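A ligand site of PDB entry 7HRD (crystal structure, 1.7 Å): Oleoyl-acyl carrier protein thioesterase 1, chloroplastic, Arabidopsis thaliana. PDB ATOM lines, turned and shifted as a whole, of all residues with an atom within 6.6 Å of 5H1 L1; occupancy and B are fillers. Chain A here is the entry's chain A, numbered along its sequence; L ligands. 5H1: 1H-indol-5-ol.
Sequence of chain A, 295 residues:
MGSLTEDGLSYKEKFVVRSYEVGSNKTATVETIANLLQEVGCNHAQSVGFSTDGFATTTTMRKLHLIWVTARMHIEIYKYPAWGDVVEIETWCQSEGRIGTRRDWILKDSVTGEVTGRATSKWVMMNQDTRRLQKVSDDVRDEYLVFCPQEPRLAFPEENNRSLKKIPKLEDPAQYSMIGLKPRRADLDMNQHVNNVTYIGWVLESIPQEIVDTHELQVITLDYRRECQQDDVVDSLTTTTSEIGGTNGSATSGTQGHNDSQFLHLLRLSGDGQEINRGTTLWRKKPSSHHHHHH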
ATOM      1  N   LEU A   9       6.455  18.301 -16.620  1.00  0.00           N
ATOM      2  CA  LEU A   9       5.553  17.238 -17.044  1.00  0.00           C
ATOM      3  C   LEU A   9       4.164  17.256 -16.383  1.00  0.00           C
ATOM      4  O   LEU A   9       3.314  16.418 -16.722  1.00  0.00           O
ATOM      5  CB  LEU A   9       6.222  15.866 -16.882  1.00  0.00           C
ATOM      6  CG  LEU A   9       7.522  15.731 -17.673  1.00  0.00           C
ATOM      7  CD1 LEU A   9       8.221  14.431 -17.343  1.00  0.00           C
ATOM      8  CD2 LEU A   9       7.249  15.831 -19.185  1.00  0.00           C
ATOM      9  N   GLY A  41      -6.502  22.454 -17.330  1.00  0.00           N
ATOM     10  CA  GLY A  41      -6.066  21.737 -18.534  1.00  0.00           C
ATOM     11  C   GLY A  41      -5.683  22.727 -19.624  1.00  0.00           C
ATOM     12  O   GLY A  41      -4.635  22.576 -20.262  1.00  0.00           O
ATOM     13  N   HIS A  44      -2.437  24.463 -18.683  1.00  0.00           N
ATOM     14  CA  HIS A  44      -1.331  23.533 -18.911  1.00  0.00           C
ATOM     15  C   HIS A  44      -0.917  23.535 -20.407  1.00  0.00           C
ATOM     16  O   HIS A  44       0.259  23.786 -20.720  1.00  0.00           O
ATOM     17  CB  HIS A  44      -1.741  22.116 -18.453  1.00  0.00           C
ATOM     18  CG  HIS A  44      -0.696  21.067 -18.661  1.00  0.00           C
ATOM     19  ND1 HIS A  44      -1.033  19.725 -18.677  1.00  0.00           N
ATOM     20  CD2 HIS A  44       0.642  21.185 -18.847  1.00  0.00           C
ATOM     21  CE1 HIS A  44       0.102  19.068 -18.857  1.00  0.00           C
ATOM     22  NE2 HIS A  44       1.144  19.902 -18.947  1.00  0.00           N
ATOM     23  N   ALA A  45      -1.871  23.345 -21.334  1.00  0.00           N
ATOM     24  CA  ALA A  45      -1.580  23.373 -22.773  1.00  0.00           C
ATOM     25  C   ALA A  45      -0.889  24.695 -23.196  1.00  0.00           C
ATOM     26  O   ALA A  45       0.147  24.669 -23.857  1.00  0.00           O
ATOM     27  CB  ALA A  45      -2.860  23.153 -23.571  1.00  0.00           C
ATOM     28  N   VAL A  48       2.814  24.916 -22.044  1.00  0.00           N
ATOM     29  CA  VAL A  48       3.759  24.078 -22.796  1.00  0.00           C
ATOM     30  C   VAL A  48       3.819  24.432 -24.291  1.00  0.00           C
ATOM     31  O   VAL A  48       4.374  23.659 -25.066  1.00  0.00           O
ATOM     32  CB  VAL A  48       3.579  22.559 -22.572  1.00  0.00           C
ATOM     33  CG1 VAL A  48       3.772  22.221 -21.090  1.00  0.00           C
ATOM     34  CG2 VAL A  48       2.235  22.050 -23.102  1.00  0.00           C
ATOM     35  N   PHE A  50       1.117  25.539 -26.557  1.00  0.00           N
ATOM     36  CA  PHE A  50      -0.051  25.514 -27.432  1.00  0.00           C
ATOM     37  C   PHE A  50      -0.673  26.914 -27.593  1.00  0.00           C
ATOM     38  O   PHE A  50      -0.922  27.597 -26.610  1.00  0.00           O
ATOM     39  CB  PHE A  50      -1.070  24.458 -26.993  1.00  0.00           C
ATOM     40  CG  PHE A  50      -0.502  23.067 -27.177  1.00  0.00           C
ATOM     41  CD1 PHE A  50      -0.545  22.449 -28.415  1.00  0.00           C
ATOM     42  CD2 PHE A  50       0.123  22.418 -26.137  1.00  0.00           C
ATOM     43  CE1 PHE A  50       0.009  21.191 -28.591  1.00  0.00           C
ATOM     44  CE2 PHE A  50       0.673  21.159 -26.321  1.00  0.00           C
ATOM     45  CZ  PHE A  50       0.601  20.551 -27.538  1.00  0.00           C
ATOM     46  N   ALA A  56      -5.602  22.504 -27.859  1.00  0.00           N
ATOM     47  CA  ALA A  56      -4.299  21.929 -27.528  1.00  0.00           C
ATOM     48  C   ALA A  56      -3.847  21.046 -28.708  1.00  0.00           C
ATOM     49  O   ALA A  56      -3.522  19.872 -28.552  1.00  0.00           O
ATOM     50  CB  ALA A  56      -4.392  21.102 -26.250  1.00  0.00           C
ATOM     51  N   THR A  57      -3.863  21.626 -29.897  1.00  0.00           N
ATOM     52  CA  THR A  57      -3.561  20.949 -31.137  1.00  0.00           C
ATOM     53  C   THR A  57      -2.159  21.209 -31.615  1.00  0.00           C
ATOM     54  O   THR A  57      -1.718  22.347 -31.650  1.00  0.00           O
ATOM     55  CB  THR A  57      -4.598  21.347 -32.185  1.00  0.00           C
ATOM     56  OG1 THR A  57      -4.613  22.767 -32.305  1.00  0.00           O
ATOM     57  CG2 THR A  57      -5.980  20.880 -31.821  1.00  0.00           C
ATOM     58  N   THR A  58      -1.466  20.134 -32.006  1.00  0.00           N
ATOM     59  CA  THR A  58      -0.101  20.214 -32.523  1.00  0.00           C
ATOM     60  C   THR A  58      -0.110  20.835 -33.933  1.00  0.00           C
ATOM     61  O   THR A  58      -1.161  20.867 -34.609  1.00  0.00           O
ATOM     62  CB  THR A  58       0.545  18.805 -32.533  1.00  0.00           C
ATOM     63  OG1 THR A  58       0.048  18.037 -33.648  1.00  0.00           O
ATOM     64  CG2 THR A  58       0.327  18.025 -31.208  1.00  0.00           C
ATOM     65  N   MET A  61      -1.584  18.531 -36.405  1.00  0.00           N
ATOM     66  CA  MET A  61      -3.028  18.429 -36.210  1.00  0.00           C
ATOM     67  C   MET A  61      -3.755  19.599 -36.897  1.00  0.00           C
ATOM     68  O   MET A  61      -4.738  19.371 -37.596  1.00  0.00           O
ATOM     69  CB  MET A  61      -3.402  18.378 -34.717  1.00  0.00           C
ATOM     70  CG  MET A  61      -3.177  17.022 -34.059  1.00  0.00           C
ATOM     71  SD  MET A  61      -3.531  17.060 -32.266  1.00  0.00           S
ATOM     72  CE  MET A  61      -5.309  16.975 -32.308  1.00  0.00           C
ATOM     73  N   TRP A  68      -8.867  17.519 -30.560  1.00  0.00           N
ATOM     74  CA  TRP A  68      -9.117  16.537 -29.501  1.00  0.00           C
ATOM     75  C   TRP A  68     -10.554  16.715 -29.057  1.00  0.00           C
ATOM     76  O   TRP A  68     -11.039  17.851 -28.912  1.00  0.00           O
ATOM     77  CB  TRP A  68      -8.178  16.739 -28.267  1.00  0.00           C
ATOM     78  CG  TRP A  68      -6.734  16.388 -28.522  1.00  0.00           C
ATOM     79  CD1 TRP A  68      -5.693  17.254 -28.614  1.00  0.00           C
ATOM     80  CD2 TRP A  68      -6.186  15.074 -28.681  1.00  0.00           C
ATOM     81  NE1 TRP A  68      -4.521  16.557 -28.795  1.00  0.00           N
ATOM     82  CE2 TRP A  68      -4.801  15.219 -28.866  1.00  0.00           C
ATOM     83  CE3 TRP A  68      -6.737  13.781 -28.670  1.00  0.00           C
ATOM     84  CZ2 TRP A  68      -3.954  14.128 -29.037  1.00  0.00           C
ATOM     85  CZ3 TRP A  68      -5.899  12.702 -28.881  1.00  0.00           C
ATOM     86  CH2 TRP A  68      -4.524  12.874 -29.063  1.00  0.00           C
ATOM     87  N   TRP A  92      -2.072  16.391 -15.677  1.00  0.00           N
ATOM     88  CA  TRP A  92      -1.066  15.864 -16.600  1.00  0.00           C
ATOM     89  C   TRP A  92      -1.753  15.049 -17.692  1.00  0.00           C
ATOM     90  O   TRP A  92      -2.919  14.655 -17.546  1.00  0.00           O
ATOM     91  CB  TRP A  92       0.011  15.069 -15.856  1.00  0.00           C
ATOM     92  CG  TRP A  92      -0.513  13.812 -15.245  1.00  0.00           C
ATOM     93  CD1 TRP A  92      -0.559  12.586 -15.811  1.00  0.00           C
ATOM     94  CD2 TRP A  92      -1.061  13.671 -13.925  1.00  0.00           C
ATOM     95  NE1 TRP A  92      -1.092  11.676 -14.926  1.00  0.00           N
ATOM     96  CE2 TRP A  92      -1.413  12.320 -13.762  1.00  0.00           C
ATOM     97  CE3 TRP A  92      -1.298  14.555 -12.862  1.00  0.00           C
ATOM     98  CZ2 TRP A  92      -1.988  11.830 -12.584  1.00  0.00           C
ATOM     99  CZ3 TRP A  92      -1.824  14.060 -11.681  1.00  0.00           C
ATOM    100  CH2 TRP A  92      -2.169  12.715 -11.553  1.00  0.00           C
ATOM    101  N   CYS A  93      -1.025  14.799 -18.780  1.00  0.00           N
ATOM    102  CA  CYS A  93      -1.514  14.024 -19.909  1.00  0.00           C
ATOM    103  C   CYS A  93      -0.633  12.846 -20.163  1.00  0.00           C
ATOM    104  O   CYS A  93       0.572  12.917 -19.962  1.00  0.00           O
ATOM    105  CB  CYS A  93      -1.584  14.888 -21.158  1.00  0.00           C
ATOM    106  SG  CYS A  93      -2.865  16.144 -21.128  1.00  0.00           S
ATOM    107  N   GLN A  94      -1.213  11.780 -20.702  1.00  0.00           N
ATOM    108  CA  GLN A  94      -0.421  10.614 -21.106  1.00  0.00           C
ATOM    109  C   GLN A  94      -0.996   9.991 -22.382  1.00  0.00           C
ATOM    110  O   GLN A  94      -2.211   9.935 -22.538  1.00  0.00           O
ATOM    111  CB  GLN A  94      -0.423   9.535 -20.010  1.00  0.00           C
ATOM    112  CG  GLN A  94       0.483   9.847 -18.834  1.00  0.00           C
ATOM    113  CD  GLN A  94       1.088   8.583 -18.309  1.00  0.00           C
ATOM    114  OE1 GLN A  94       0.386   7.652 -17.904  1.00  0.00           O
ATOM    115  NE2 GLN A  94       2.413   8.531 -18.297  1.00  0.00           N
ATOM    116  N   SER A  95      -0.126   9.467 -23.273  1.00  0.00           N
ATOM    117  CA  SER A  95      -0.573   8.789 -24.489  1.00  0.00           C
ATOM    118  C   SER A  95      -1.104   7.389 -24.113  1.00  0.00           C
ATOM    119  O   SER A  95      -0.515   6.721 -23.261  1.00  0.00           O
ATOM    120  CB  SER A  95       0.605   8.614 -25.445  1.00  0.00           C
ATOM    121  OG  SER A  95       0.247   8.491 -26.814  1.00  0.00           O
ATOM    122  N   THR A 101      -5.410  10.084 -26.070  1.00  0.00           N
ATOM    123  CA  THR A 101      -4.753  10.527 -24.847  1.00  0.00           C
ATOM    124  C   THR A 101      -5.695  10.511 -23.638  1.00  0.00           C
ATOM    125  O   THR A 101      -6.928  10.457 -23.777  1.00  0.00           O
ATOM    126  CB  THR A 101      -4.049  11.900 -25.052  1.00  0.00           C
ATOM    127  OG1 THR A 101      -5.038  12.875 -25.388  1.00  0.00           O
ATOM    128  CG2 THR A 101      -2.957  11.871 -26.080  1.00  0.00           C
ATOM    129  N   ARG A 103      -6.207  12.668 -19.907  1.00  0.00           N
ATOM    130  CA  ARG A 103      -5.803  13.763 -19.043  1.00  0.00           C
ATOM    131  C   ARG A 103      -6.330  13.391 -17.665  1.00  0.00           C
ATOM    132  O   ARG A 103      -7.519  13.045 -17.556  1.00  0.00           O
ATOM    133  CB  ARG A 103      -6.370  15.126 -19.439  1.00  0.00           C
ATOM    134  CG  ARG A 103      -6.015  16.247 -18.449  1.00  0.00           C
ATOM    135  CD  ARG A 103      -6.342  17.633 -18.993  1.00  0.00           C
ATOM    136  NE  ARG A 103      -5.449  18.058 -20.077  1.00  0.00           N
ATOM    137  CZ  ARG A 103      -4.215  18.545 -19.890  1.00  0.00           C
ATOM    138  NH1 ARG A 103      -3.466  18.905 -20.935  1.00  0.00           N
ATOM    139  NH2 ARG A 103      -3.700  18.640 -18.667  1.00  0.00           N
ATOM    140  N   TYR A 144       3.651  15.433 -29.304  1.00  0.00           N
ATOM    141  CA  TYR A 144       3.134  15.684 -27.955  1.00  0.00           C
ATOM    142  C   TYR A 144       3.710  14.768 -26.868  1.00  0.00           C
ATOM    143  O   TYR A 144       3.443  14.993 -25.691  1.00  0.00           O
ATOM    144  CB  TYR A 144       1.598  15.688 -27.913  1.00  0.00           C
ATOM    145  CG  TYR A 144       0.935  14.371 -28.222  1.00  0.00           C
ATOM    146  CD1 TYR A 144       1.015  13.297 -27.341  1.00  0.00           C
ATOM    147  CD2 TYR A 144       0.097  14.227 -29.327  1.00  0.00           C
ATOM    148  CE1 TYR A 144       0.355  12.103 -27.583  1.00  0.00           C
ATOM    149  CE2 TYR A 144      -0.562  13.035 -29.591  1.00  0.00           C
ATOM    150  CZ  TYR A 144      -0.440  11.975 -28.706  1.00  0.00           C
ATOM    151  OH  TYR A 144      -1.087  10.785 -28.942  1.00  0.00           O
ATOM    152  N   LEU A 145       4.525  13.757 -27.236  1.00  0.00           N
ATOM    153  CA  LEU A 145       5.140  12.854 -26.263  1.00  0.00           C
ATOM    154  C   LEU A 145       6.103  13.587 -25.306  1.00  0.00           C
ATOM    155  O   LEU A 145       6.204  13.239 -24.110  1.00  0.00           O
ATOM    156  CB  LEU A 145       5.870  11.723 -26.977  1.00  0.00           C
ATOM    157  CG  LEU A 145       5.022  10.510 -27.274  1.00  0.00           C
ATOM    158  CD1 LEU A 145       5.766   9.565 -28.252  1.00  0.00           C
ATOM    159  CD2 LEU A 145       4.652   9.795 -25.979  1.00  0.00           C
ATOM    160  N   PHE A 147       5.705  16.290 -23.899  1.00  0.00           N
ATOM    161  CA  PHE A 147       4.915  16.970 -22.865  1.00  0.00           C
ATOM    162  C   PHE A 147       4.259  16.006 -21.853  1.00  0.00           C
ATOM    163  O   PHE A 147       3.550  16.449 -20.957  1.00  0.00           O
ATOM    164  CB  PHE A 147       3.823  17.838 -23.521  1.00  0.00           C
ATOM    165  CG  PHE A 147       4.372  18.766 -24.575  1.00  0.00           C
ATOM    166  CD1 PHE A 147       5.404  19.642 -24.288  1.00  0.00           C
ATOM    167  CD2 PHE A 147       3.925  18.692 -25.891  1.00  0.00           C
ATOM    168  CE1 PHE A 147       5.947  20.456 -25.269  1.00  0.00           C
ATOM    169  CE2 PHE A 147       4.452  19.522 -26.866  1.00  0.00           C
ATOM    170  CZ  PHE A 147       5.462  20.398 -26.549  1.00  0.00           C
ATOM    171  N   CYS A 148       4.499  14.698 -22.000  1.00  0.00           N
ATOM    172  CA  CYS A 148       3.895  13.694 -21.178  1.00  0.00           C
ATOM    173  C   CYS A 148       4.936  12.947 -20.392  1.00  0.00           C
ATOM    174  O   CYS A 148       6.001  12.623 -20.929  1.00  0.00           O
ATOM    175  CB  CYS A 148       3.096  12.725 -22.046  1.00  0.00           C
ATOM    176  SG  CYS A 148       1.881  13.510 -23.133  1.00  0.00           S
HETATM  177  O10 5H1 L   1      -2.046  17.172 -27.380  1.00  0.00           O
HETATM  178  C5  5H1 L   1      -1.489  17.153 -26.134  1.00  0.00           C
HETATM  179  C6  5H1 L   1      -1.075  15.916 -25.601  1.00  0.00           C
HETATM  180  C7  5H1 L   1      -0.404  15.845 -24.407  1.00  0.00           C
HETATM  181  C8  5H1 L   1      -0.252  17.022 -23.686  1.00  0.00           C
HETATM  182  N1  5H1 L   1       0.334  17.259 -22.466  1.00  0.00           N
HETATM  183  C4  5H1 L   1      -1.345  18.317 -25.420  1.00  0.00           C
HETATM  184  C9  5H1 L   1      -0.725  18.265 -24.164  1.00  0.00           C
HETATM  185  C3  5H1 L   1      -0.391  19.252 -23.181  1.00  0.00           C
HETATM  186  C2  5H1 L   1       0.243  18.586 -22.164  1.00  0.00           C
HETATM  187  O10 5H1 L   2     -10.797  19.749 -20.105  1.00  0.00           O
HETATM  188  C5  5H1 L   2     -10.018  20.477 -20.958  1.00  0.00           C
HETATM  189  C6  5H1 L   2     -10.633  21.461 -21.742  1.00  0.00           C
HETATM  190  C7  5H1 L   2      -9.919  22.212 -22.646  1.00  0.00           C
HETATM  191  C8  5H1 L   2      -8.556  21.960 -22.756  1.00  0.00           C
HETATM  192  N1  5H1 L   2      -7.592  22.547 -23.544  1.00  0.00           N
HETATM  193  C4  5H1 L   2      -8.681  20.215 -21.057  1.00  0.00           C
HETATM  194  C9  5H1 L   2      -7.917  20.964 -21.980  1.00  0.00           C
HETATM  195  C3  5H1 L   2      -6.537  20.984 -22.350  1.00  0.00           C
HETATM  196  C2  5H1 L   2      -6.387  21.942 -23.282  1.00  0.00           C
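O10 of 5H1 L1 lies within hydrogen-bond range of O of Ala 56, 3.3 Å away.
N1 of 5H1 L1 lies close to SG of Cys 93, at 3.6 Å.
NE1 of Trp 68 sits at hydrogen-bond distance from O10 of 5H1 L1 (2.9 Å).
NE1 of Trp 68 sits close to SD of Met 61, 3.6 Å away.
The side-chain hydroxyl of Tyr 144 lies within hydrogen-bond range of the side-chain hydroxyl of Ser 95.
The backbone NH (N) of Phe 50 lies within hydrogen-bond range of the backbone carbonyl oxygen (O) of Ala 45, at 3.0 Å.
The backbone carbonyl oxygen (O) of Ala 56 lies close to the indole nitrogen (NE1) of Trp 68.
O of Cys 93 sits close to SG of Cys 148 (3.5 Å).
A ring nitrogen (ND1) of His 44 sits at hydrogen-bond distance from the guanidinium group of Arg 103, 2.9 Å away.
SG of Cys 93 is in hydrogen-bond range of NH1 of Arg 103, at 2.8 Å.
SG of Cys 148 is in hydrogen-bond range of O of Tyr 144, 3.3 Å away.
Residues that only touch 5H1 L1: His 44, Cys 148, Tyr 144, Phe 50, Phe 147, Arg 103 and Val 48.
Hydrophobic or aromatic side chains that line 5H1 L1: His 44, Val 48, Phe 50, Trp 68, Tyr 144 and Phe 147.
Of the 21 residues printed, 10 come within 4 Å of 5H1 L1.
The nearest printed residue that does not touch 5H1 L1 is Ala 45 (4.3 Å).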
